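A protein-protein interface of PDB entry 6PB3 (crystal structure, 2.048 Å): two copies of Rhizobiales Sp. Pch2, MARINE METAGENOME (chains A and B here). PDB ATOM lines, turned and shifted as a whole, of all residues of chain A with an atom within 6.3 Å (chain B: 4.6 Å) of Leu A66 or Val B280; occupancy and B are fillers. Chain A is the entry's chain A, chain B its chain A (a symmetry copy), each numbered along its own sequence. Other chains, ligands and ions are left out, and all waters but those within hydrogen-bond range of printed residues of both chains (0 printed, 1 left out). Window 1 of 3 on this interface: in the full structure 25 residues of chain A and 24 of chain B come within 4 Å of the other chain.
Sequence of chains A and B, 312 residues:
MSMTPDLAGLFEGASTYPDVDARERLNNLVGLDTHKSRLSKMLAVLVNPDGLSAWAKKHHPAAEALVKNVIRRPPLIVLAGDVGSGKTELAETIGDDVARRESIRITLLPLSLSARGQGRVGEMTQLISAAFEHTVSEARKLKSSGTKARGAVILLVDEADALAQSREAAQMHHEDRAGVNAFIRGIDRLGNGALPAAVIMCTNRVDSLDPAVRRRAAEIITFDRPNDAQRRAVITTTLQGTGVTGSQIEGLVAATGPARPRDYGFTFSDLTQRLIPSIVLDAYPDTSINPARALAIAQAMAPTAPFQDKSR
The backbone carbonyl oxygen (O) of Ala A65 lies within hydrogen-bond range of the side-chain amide nitrogen (ND2) of Asn A69 (3.4 Å).
OD1 of Asn A69 lies close to O of Leu A66 (3.2 Å).
Among the printed residues, pairs that only touch across the chains: His A60 with Ile B289 (3.2 Å), Leu A66 with Thr B238 (3.5 Å), His A60 with Thr B242 (3.5 Å), Leu A52 with Tyr B284 (3.6 Å), Leu A66 with Ile B289 (3.6 Å), Trp A55 with Ala B283 (3.7 Å), Asn A69 with Thr B238 (3.8 Å), Leu A66 with Val B280 (3.8 Å), Trp A55 with Tyr B284 (3.9 Å), Leu A66 with Thr B242 (3.9 Å), Leu A52 with Val B280 (3.97 Å) and Trp A55 with Ile B289 (3.995 Å).
Leu A66 touches four residues of chain B.
Of chain A, only Leu A52 and Leu A66 come within 4 Å of Val B280.
Of the printed residues of chain B, Trp A55 touches Ala B283 (3.7 Å), Tyr B284 (3.9 Å) and Ile B289 (3.995 Å).
Printed residues of chain A within 4 Å of Tyr B284: Leu A52 (3.6 Å) and Trp A55 (3.9 Å).
Of the printed residues of chain A, Thr B242 touches His A60 and Leu A66.
Of the printed residues of chain A, Thr B238 touches Leu A66 (3.5 Å) and Asn A69 (3.8 Å).
Ala A65 touches none of the printed residues of chain B.
Asp B282 touches none of the printed residues of chain A.
The nearest printed residue of chain B that does not touch Leu A66 is Ile B276 (5.1 Å).
Hydrophobic or aromatic side chains of chain A that line the printed part of chain B: Leu A52, Trp A55, His A60 and Leu A66.
Printed residues of chain B that touch a printed residue of chain A: Thr B238, Thr B242, Val B280, Ala B283, Tyr B284 and Ile B289.
Among the printed residues, 12 pairs touch across the chains.
No position is printed for both chains.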
ATOM      1  N   LEU A  52     -11.809   9.026 -18.811  1.00  0.00           N
ATOM      2  CA  LEU A  52     -12.066  10.115 -17.869  1.00  0.00           C
ATOM      3  C   LEU A  52     -13.549  10.209 -17.534  1.00  0.00           C
ATOM      4  O   LEU A  52     -13.920  10.407 -16.370  1.00  0.00           O
ATOM      5  CB  LEU A  52     -11.571  11.448 -18.436  1.00  0.00           C
ATOM      6  CG  LEU A  52     -11.718  12.664 -17.514  1.00  0.00           C
ATOM      7  CD1 LEU A  52     -10.886  12.467 -16.244  1.00  0.00           C
ATOM      8  CD2 LEU A  52     -11.296  13.944 -18.227  1.00  0.00           C
ATOM      9  N   TRP A  55     -14.314   7.389 -15.106  1.00  0.00           N
ATOM     10  CA  TRP A  55     -13.835   7.741 -13.771  1.00  0.00           C
ATOM     11  C   TRP A  55     -14.764   8.739 -13.095  1.00  0.00           C
ATOM     12  O   TRP A  55     -15.087   8.588 -11.912  1.00  0.00           O
ATOM     13  CB  TRP A  55     -12.417   8.307 -13.832  1.00  0.00           C
ATOM     14  CG  TRP A  55     -12.039   8.992 -12.548  1.00  0.00           C
ATOM     15  CD1 TRP A  55     -11.515   8.410 -11.434  1.00  0.00           C
ATOM     16  CD2 TRP A  55     -12.193  10.385 -12.238  1.00  0.00           C
ATOM     17  NE1 TRP A  55     -11.318   9.353 -10.453  1.00  0.00           N
ATOM     18  CE2 TRP A  55     -11.727  10.573 -10.920  1.00  0.00           C
ATOM     19  CE3 TRP A  55     -12.671  11.491 -12.948  1.00  0.00           C
ATOM     20  CZ2 TRP A  55     -11.723  11.822 -10.298  1.00  0.00           C
ATOM     21  CZ3 TRP A  55     -12.674  12.735 -12.322  1.00  0.00           C
ATOM     22  CH2 TRP A  55     -12.203  12.886 -11.011  1.00  0.00           C
ATOM     23  N   ALA A  56     -15.211   9.760 -13.835  1.00  0.00           N
ATOM     24  CA  ALA A  56     -16.105  10.765 -13.261  1.00  0.00           C
ATOM     25  C   ALA A  56     -17.401  10.144 -12.770  1.00  0.00           C
ATOM     26  O   ALA A  56     -17.874  10.467 -11.675  1.00  0.00           O
ATOM     27  CB  ALA A  56     -16.403  11.861 -14.283  1.00  0.00           C
ATOM     28  N   HIS A  60     -17.669  10.682  -9.038  1.00  0.00           N
ATOM     29  CA  HIS A  60     -18.402  11.938  -8.848  1.00  0.00           C
ATOM     30  C   HIS A  60     -19.508  12.056  -9.886  1.00  0.00           C
ATOM     31  O   HIS A  60     -19.458  12.911 -10.776  1.00  0.00           O
ATOM     32  CB  HIS A  60     -17.454  13.137  -8.934  1.00  0.00           C
ATOM     33  CG  HIS A  60     -16.331  13.096  -7.945  1.00  0.00           C
ATOM     34  ND1 HIS A  60     -15.017  12.909  -8.319  1.00  0.00           N
ATOM     35  CD2 HIS A  60     -16.326  13.209  -6.596  1.00  0.00           C
ATOM     36  CE1 HIS A  60     -14.250  12.913  -7.244  1.00  0.00           C
ATOM     37  NE2 HIS A  60     -15.020  13.090  -6.185  1.00  0.00           N
ATOM     38  N   ALA A  63     -21.164  15.402 -10.723  1.00  0.00           N
ATOM     39  CA  ALA A  63     -20.303  16.477 -11.205  1.00  0.00           C
ATOM     40  C   ALA A  63     -20.692  16.857 -12.627  1.00  0.00           C
ATOM     41  O   ALA A  63     -20.657  16.023 -13.538  1.00  0.00           O
ATOM     42  CB  ALA A  63     -18.836  16.062 -11.141  1.00  0.00           C
ATOM     43  N   GLU A  64     -21.048  18.124 -12.818  1.00  0.00           N
ATOM     44  CA  GLU A  64     -21.557  18.608 -14.093  1.00  0.00           C
ATOM     45  C   GLU A  64     -20.464  19.186 -14.983  1.00  0.00           C
ATOM     46  O   GLU A  64     -20.387  18.857 -16.170  1.00  0.00           O
ATOM     47  CB  GLU A  64     -22.643  19.655 -13.839  1.00  0.00           C
ATOM     48  CG  GLU A  64     -23.786  19.607 -14.825  1.00  0.00           C
ATOM     49  CD  GLU A  64     -25.038  20.235 -14.262  1.00  0.00           C
ATOM     50  OE1 GLU A  64     -25.199  20.231 -13.022  1.00  0.00           O
ATOM     51  OE2 GLU A  64     -25.859  20.737 -15.056  1.00  0.00           O
ATOM     52  N   ALA A  65     -19.605  20.038 -14.431  1.00  0.00           N
ATOM     53  CA  ALA A  65     -18.544  20.665 -15.204  1.00  0.00           C
ATOM     54  C   ALA A  65     -17.162  20.168 -14.814  1.00  0.00           C
ATOM     55  O   ALA A  65     -16.164  20.742 -15.264  1.00  0.00           O
ATOM     56  CB  ALA A  65     -18.612  22.185 -15.061  1.00  0.00           C
ATOM     57  N   LEU A  66     -17.075  19.112 -14.002  1.00  0.00           N
ATOM     58  CA  LEU A  66     -15.779  18.657 -13.507  1.00  0.00           C
ATOM     59  C   LEU A  66     -14.848  18.272 -14.648  1.00  0.00           C
ATOM     60  O   LEU A  66     -13.686  18.692 -14.687  1.00  0.00           O
ATOM     61  CB  LEU A  66     -15.962  17.477 -12.553  1.00  0.00           C
ATOM     62  CG  LEU A  66     -14.694  16.725 -12.140  1.00  0.00           C
ATOM     63  CD1 LEU A  66     -13.700  17.658 -11.472  1.00  0.00           C
ATOM     64  CD2 LEU A  66     -15.053  15.570 -11.203  1.00  0.00           C
ATOM     65  N   VAL A  67     -15.336  17.459 -15.579  1.00  0.00           N
ATOM     66  CA  VAL A  67     -14.526  17.014 -16.706  1.00  0.00           C
ATOM     67  C   VAL A  67     -14.972  17.622 -18.022  1.00  0.00           C
ATOM     68  O   VAL A  67     -14.249  17.481 -19.024  1.00  0.00           O
ATOM     69  CB  VAL A  67     -14.514  15.476 -16.820  1.00  0.00           C
ATOM     70  CG1 VAL A  67     -13.916  14.864 -15.571  1.00  0.00           C
ATOM     71  CG2 VAL A  67     -15.919  14.966 -17.048  1.00  0.00           C
ATOM     72  N   LYS A  68     -16.137  18.283 -18.059  1.00  0.00           N
ATOM     73  CA  LYS A  68     -16.611  18.887 -19.299  1.00  0.00           C
ATOM     74  C   LYS A  68     -15.556  19.802 -19.899  1.00  0.00           C
ATOM     75  O   LYS A  68     -15.374  19.837 -21.120  1.00  0.00           O
ATOM     76  CB  LYS A  68     -17.911  19.660 -19.052  1.00  0.00           C
ATOM     77  N   ASN A  69     -14.835  20.537 -19.049  1.00  0.00           N
ATOM     78  CA  ASN A  69     -13.767  21.388 -19.557  1.00  0.00           C
ATOM     79  C   ASN A  69     -12.582  20.564 -20.048  1.00  0.00           C
ATOM     80  O   ASN A  69     -12.014  20.870 -21.102  1.00  0.00           O
ATOM     81  CB  ASN A  69     -13.335  22.398 -18.488  1.00  0.00           C
ATOM     82  CG  ASN A  69     -13.134  21.768 -17.118  1.00  0.00           C
ATOM     83  OD1 ASN A  69     -12.734  20.609 -17.004  1.00  0.00           O
ATOM     84  ND2 ASN A  69     -13.413  22.535 -16.069  1.00  0.00           N
ATOM     85  N   VAL A  70     -12.211  19.499 -19.327  1.00  0.00           N
ATOM     86  CA  VAL A  70     -10.966  18.790 -19.635  1.00  0.00           C
ATOM     87  C   VAL A  70     -11.074  18.031 -20.953  1.00  0.00           C
ATOM     88  O   VAL A  70     -10.106  17.943 -21.716  1.00  0.00           O
ATOM     89  CB  VAL A  70     -10.583  17.841 -18.484  1.00  0.00           C
ATOM     90  CG1 VAL A  70      -9.381  17.008 -18.867  1.00  0.00           C
ATOM     91  CG2 VAL A  70     -10.294  18.613 -17.236  1.00  0.00           C
ATOM     92  N   THR B 238     -16.175  24.308 -11.118  1.00  0.00           N
ATOM     93  CA  THR B 238     -15.473  23.092 -11.520  1.00  0.00           C
ATOM     94  C   THR B 238     -15.616  21.993 -10.472  1.00  0.00           C
ATOM     95  O   THR B 238     -15.781  20.816 -10.816  1.00  0.00           O
ATOM     96  CB  THR B 238     -13.996  23.395 -11.781  1.00  0.00           C
ATOM     97  OG1 THR B 238     -13.892  24.406 -12.795  1.00  0.00           O
ATOM     98  CG2 THR B 238     -13.284  22.155 -12.256  1.00  0.00           C
ATOM     99  N   THR B 242     -18.271  17.341  -6.150  1.00  0.00           N
ATOM    100  CA  THR B 242     -17.155  16.534  -5.683  1.00  0.00           C
ATOM    101  C   THR B 242     -17.082  16.469  -4.169  1.00  0.00           C
ATOM    102  O   THR B 242     -16.227  15.758  -3.637  1.00  0.00           O
ATOM    103  CB  THR B 242     -15.829  17.077  -6.220  1.00  0.00           C
ATOM    104  OG1 THR B 242     -15.598  18.380  -5.671  1.00  0.00           O
ATOM    105  CG2 THR B 242     -15.847  17.162  -7.740  1.00  0.00           C
ATOM    106  N   ILE B 276      -6.537  23.254 -12.846  1.00  0.00           N
ATOM    107  CA  ILE B 276      -7.698  22.364 -12.971  1.00  0.00           C
ATOM    108  C   ILE B 276      -7.301  20.993 -13.523  1.00  0.00           C
ATOM    109  O   ILE B 276      -7.611  19.980 -12.879  1.00  0.00           O
ATOM    110  CB  ILE B 276      -8.813  23.040 -13.776  1.00  0.00           C
ATOM    111  CG1 ILE B 276      -9.561  24.071 -12.910  1.00  0.00           C
ATOM    112  CG2 ILE B 276      -9.803  21.982 -14.302  1.00  0.00           C
ATOM    113  CD1 ILE B 276     -10.438  25.005 -13.726  1.00  0.00           C
ATOM    114  N   PRO B 277      -6.594  20.884 -14.652  1.00  0.00           N
ATOM    115  CA  PRO B 277      -6.152  19.553 -15.081  1.00  0.00           C
ATOM    116  C   PRO B 277      -5.364  18.817 -14.016  1.00  0.00           C
ATOM    117  O   PRO B 277      -5.599  17.619 -13.814  1.00  0.00           O
ATOM    118  CB  PRO B 277      -5.286  19.859 -16.319  1.00  0.00           C
ATOM    119  CG  PRO B 277      -5.756  21.112 -16.851  1.00  0.00           C
ATOM    120  CD  PRO B 277      -6.194  21.919 -15.625  1.00  0.00           C
ATOM    121  N   SER B 278      -4.435  19.501 -13.328  1.00  0.00           N
ATOM    122  CA  SER B 278      -3.595  18.831 -12.340  1.00  0.00           C
ATOM    123  C   SER B 278      -4.440  18.247 -11.221  1.00  0.00           C
ATOM    124  O   SER B 278      -4.139  17.171 -10.702  1.00  0.00           O
ATOM    125  CB  SER B 278      -2.560  19.803 -11.757  1.00  0.00           C
ATOM    126  OG  SER B 278      -1.688  20.310 -12.762  1.00  0.00           O
ATOM    127  N   ILE B 279      -5.464  18.978 -10.787  1.00  0.00           N
ATOM    128  CA  ILE B 279      -6.296  18.483  -9.702  1.00  0.00           C
ATOM    129  C   ILE B 279      -7.059  17.245 -10.148  1.00  0.00           C
ATOM    130  O   ILE B 279      -7.093  16.228  -9.444  1.00  0.00           O
ATOM    131  CB  ILE B 279      -7.241  19.588  -9.210  1.00  0.00           C
ATOM    132  CG1 ILE B 279      -6.435  20.629  -8.442  1.00  0.00           C
ATOM    133  CG2 ILE B 279      -8.332  18.986  -8.341  1.00  0.00           C
ATOM    134  CD1 ILE B 279      -7.247  21.817  -8.027  1.00  0.00           C
ATOM    135  N   VAL B 280      -7.653  17.300 -11.341  1.00  0.00           N
ATOM    136  CA  VAL B 280      -8.423  16.165 -11.849  1.00  0.00           C
ATOM    137  C   VAL B 280      -7.516  14.966 -12.104  1.00  0.00           C
ATOM    138  O   VAL B 280      -7.788  13.846 -11.650  1.00  0.00           O
ATOM    139  CB  VAL B 280      -9.177  16.570 -13.126  1.00  0.00           C
ATOM    140  CG1 VAL B 280      -9.893  15.357 -13.709  1.00  0.00           C
ATOM    141  CG2 VAL B 280     -10.142  17.699 -12.828  1.00  0.00           C
ATOM    142  N   LEU B 281      -6.425  15.177 -12.845  1.00  0.00           N
ATOM    143  CA  LEU B 281      -5.554  14.059 -13.196  1.00  0.00           C
ATOM    144  C   LEU B 281      -4.933  13.427 -11.962  1.00  0.00           C
ATOM    145  O   LEU B 281      -4.607  12.233 -11.970  1.00  0.00           O
ATOM    146  CB  LEU B 281      -4.466  14.526 -14.159  1.00  0.00           C
ATOM    147  CG  LEU B 281      -4.982  15.032 -15.503  1.00  0.00           C
ATOM    148  CD1 LEU B 281      -3.817  15.385 -16.402  1.00  0.00           C
ATOM    149  CD2 LEU B 281      -5.863  13.987 -16.146  1.00  0.00           C
ATOM    150  N   ASP B 282      -4.758  14.204 -10.891  1.00  0.00           N
ATOM    151  CA  ASP B 282      -4.179  13.636  -9.676  1.00  0.00           C
ATOM    152  C   ASP B 282      -5.043  12.520  -9.105  1.00  0.00           C
ATOM    153  O   ASP B 282      -4.519  11.539  -8.564  1.00  0.00           O
ATOM    154  CB  ASP B 282      -3.973  14.720  -8.624  1.00  0.00           C
ATOM    155  CG  ASP B 282      -3.475  14.162  -7.321  1.00  0.00           C
ATOM    156  OD1 ASP B 282      -2.275  13.822  -7.259  1.00  0.00           O
ATOM    157  OD2 ASP B 282      -4.277  14.048  -6.370  1.00  0.00           O
ATOM    158  N   ALA B 283      -6.362  12.647  -9.219  1.00  0.00           N
ATOM    159  CA  ALA B 283      -7.277  11.617  -8.748  1.00  0.00           C
ATOM    160  C   ALA B 283      -7.527  10.546  -9.796  1.00  0.00           C
ATOM    161  O   ALA B 283      -7.570   9.361  -9.460  1.00  0.00           O
ATOM    162  CB  ALA B 283      -8.602  12.258  -8.345  1.00  0.00           C
ATOM    163  N   TYR B 284      -7.680  10.951 -11.054  1.00  0.00           N
ATOM    164  CA  TYR B 284      -7.897  10.014 -12.146  1.00  0.00           C
ATOM    165  C   TYR B 284      -6.756   9.000 -12.197  1.00  0.00           C
ATOM    166  O   TYR B 284      -5.593   9.366 -11.982  1.00  0.00           O
ATOM    167  CB  TYR B 284      -8.004  10.790 -13.469  1.00  0.00           C
ATOM    168  CG  TYR B 284      -7.867   9.977 -14.747  1.00  0.00           C
ATOM    169  CD1 TYR B 284      -8.989   9.491 -15.409  1.00  0.00           C
ATOM    170  CD2 TYR B 284      -6.618   9.734 -15.315  1.00  0.00           C
ATOM    171  CE1 TYR B 284      -8.867   8.765 -16.587  1.00  0.00           C
ATOM    172  CE2 TYR B 284      -6.492   9.004 -16.490  1.00  0.00           C
ATOM    173  CZ  TYR B 284      -7.618   8.527 -17.122  1.00  0.00           C
ATOM    174  OH  TYR B 284      -7.498   7.798 -18.284  1.00  0.00           O
ATOM    175  N   ILE B 289     -11.444  12.814  -5.791  1.00  0.00           N
ATOM    176  CA  ILE B 289     -10.730  14.074  -5.625  1.00  0.00           C
ATOM    177  C   ILE B 289     -10.415  14.301  -4.151  1.00  0.00           C
ATOM    178  O   ILE B 289     -11.274  14.132  -3.278  1.00  0.00           O
ATOM    179  CB  ILE B 289     -11.554  15.221  -6.231  1.00  0.00           C
ATOM    180  CG1 ILE B 289     -11.363  15.239  -7.749  1.00  0.00           C
ATOM    181  CG2 ILE B 289     -11.151  16.563  -5.646  1.00  0.00           C
ATOM    182  CD1 ILE B 289     -12.425  15.980  -8.493  1.00  0.00           C
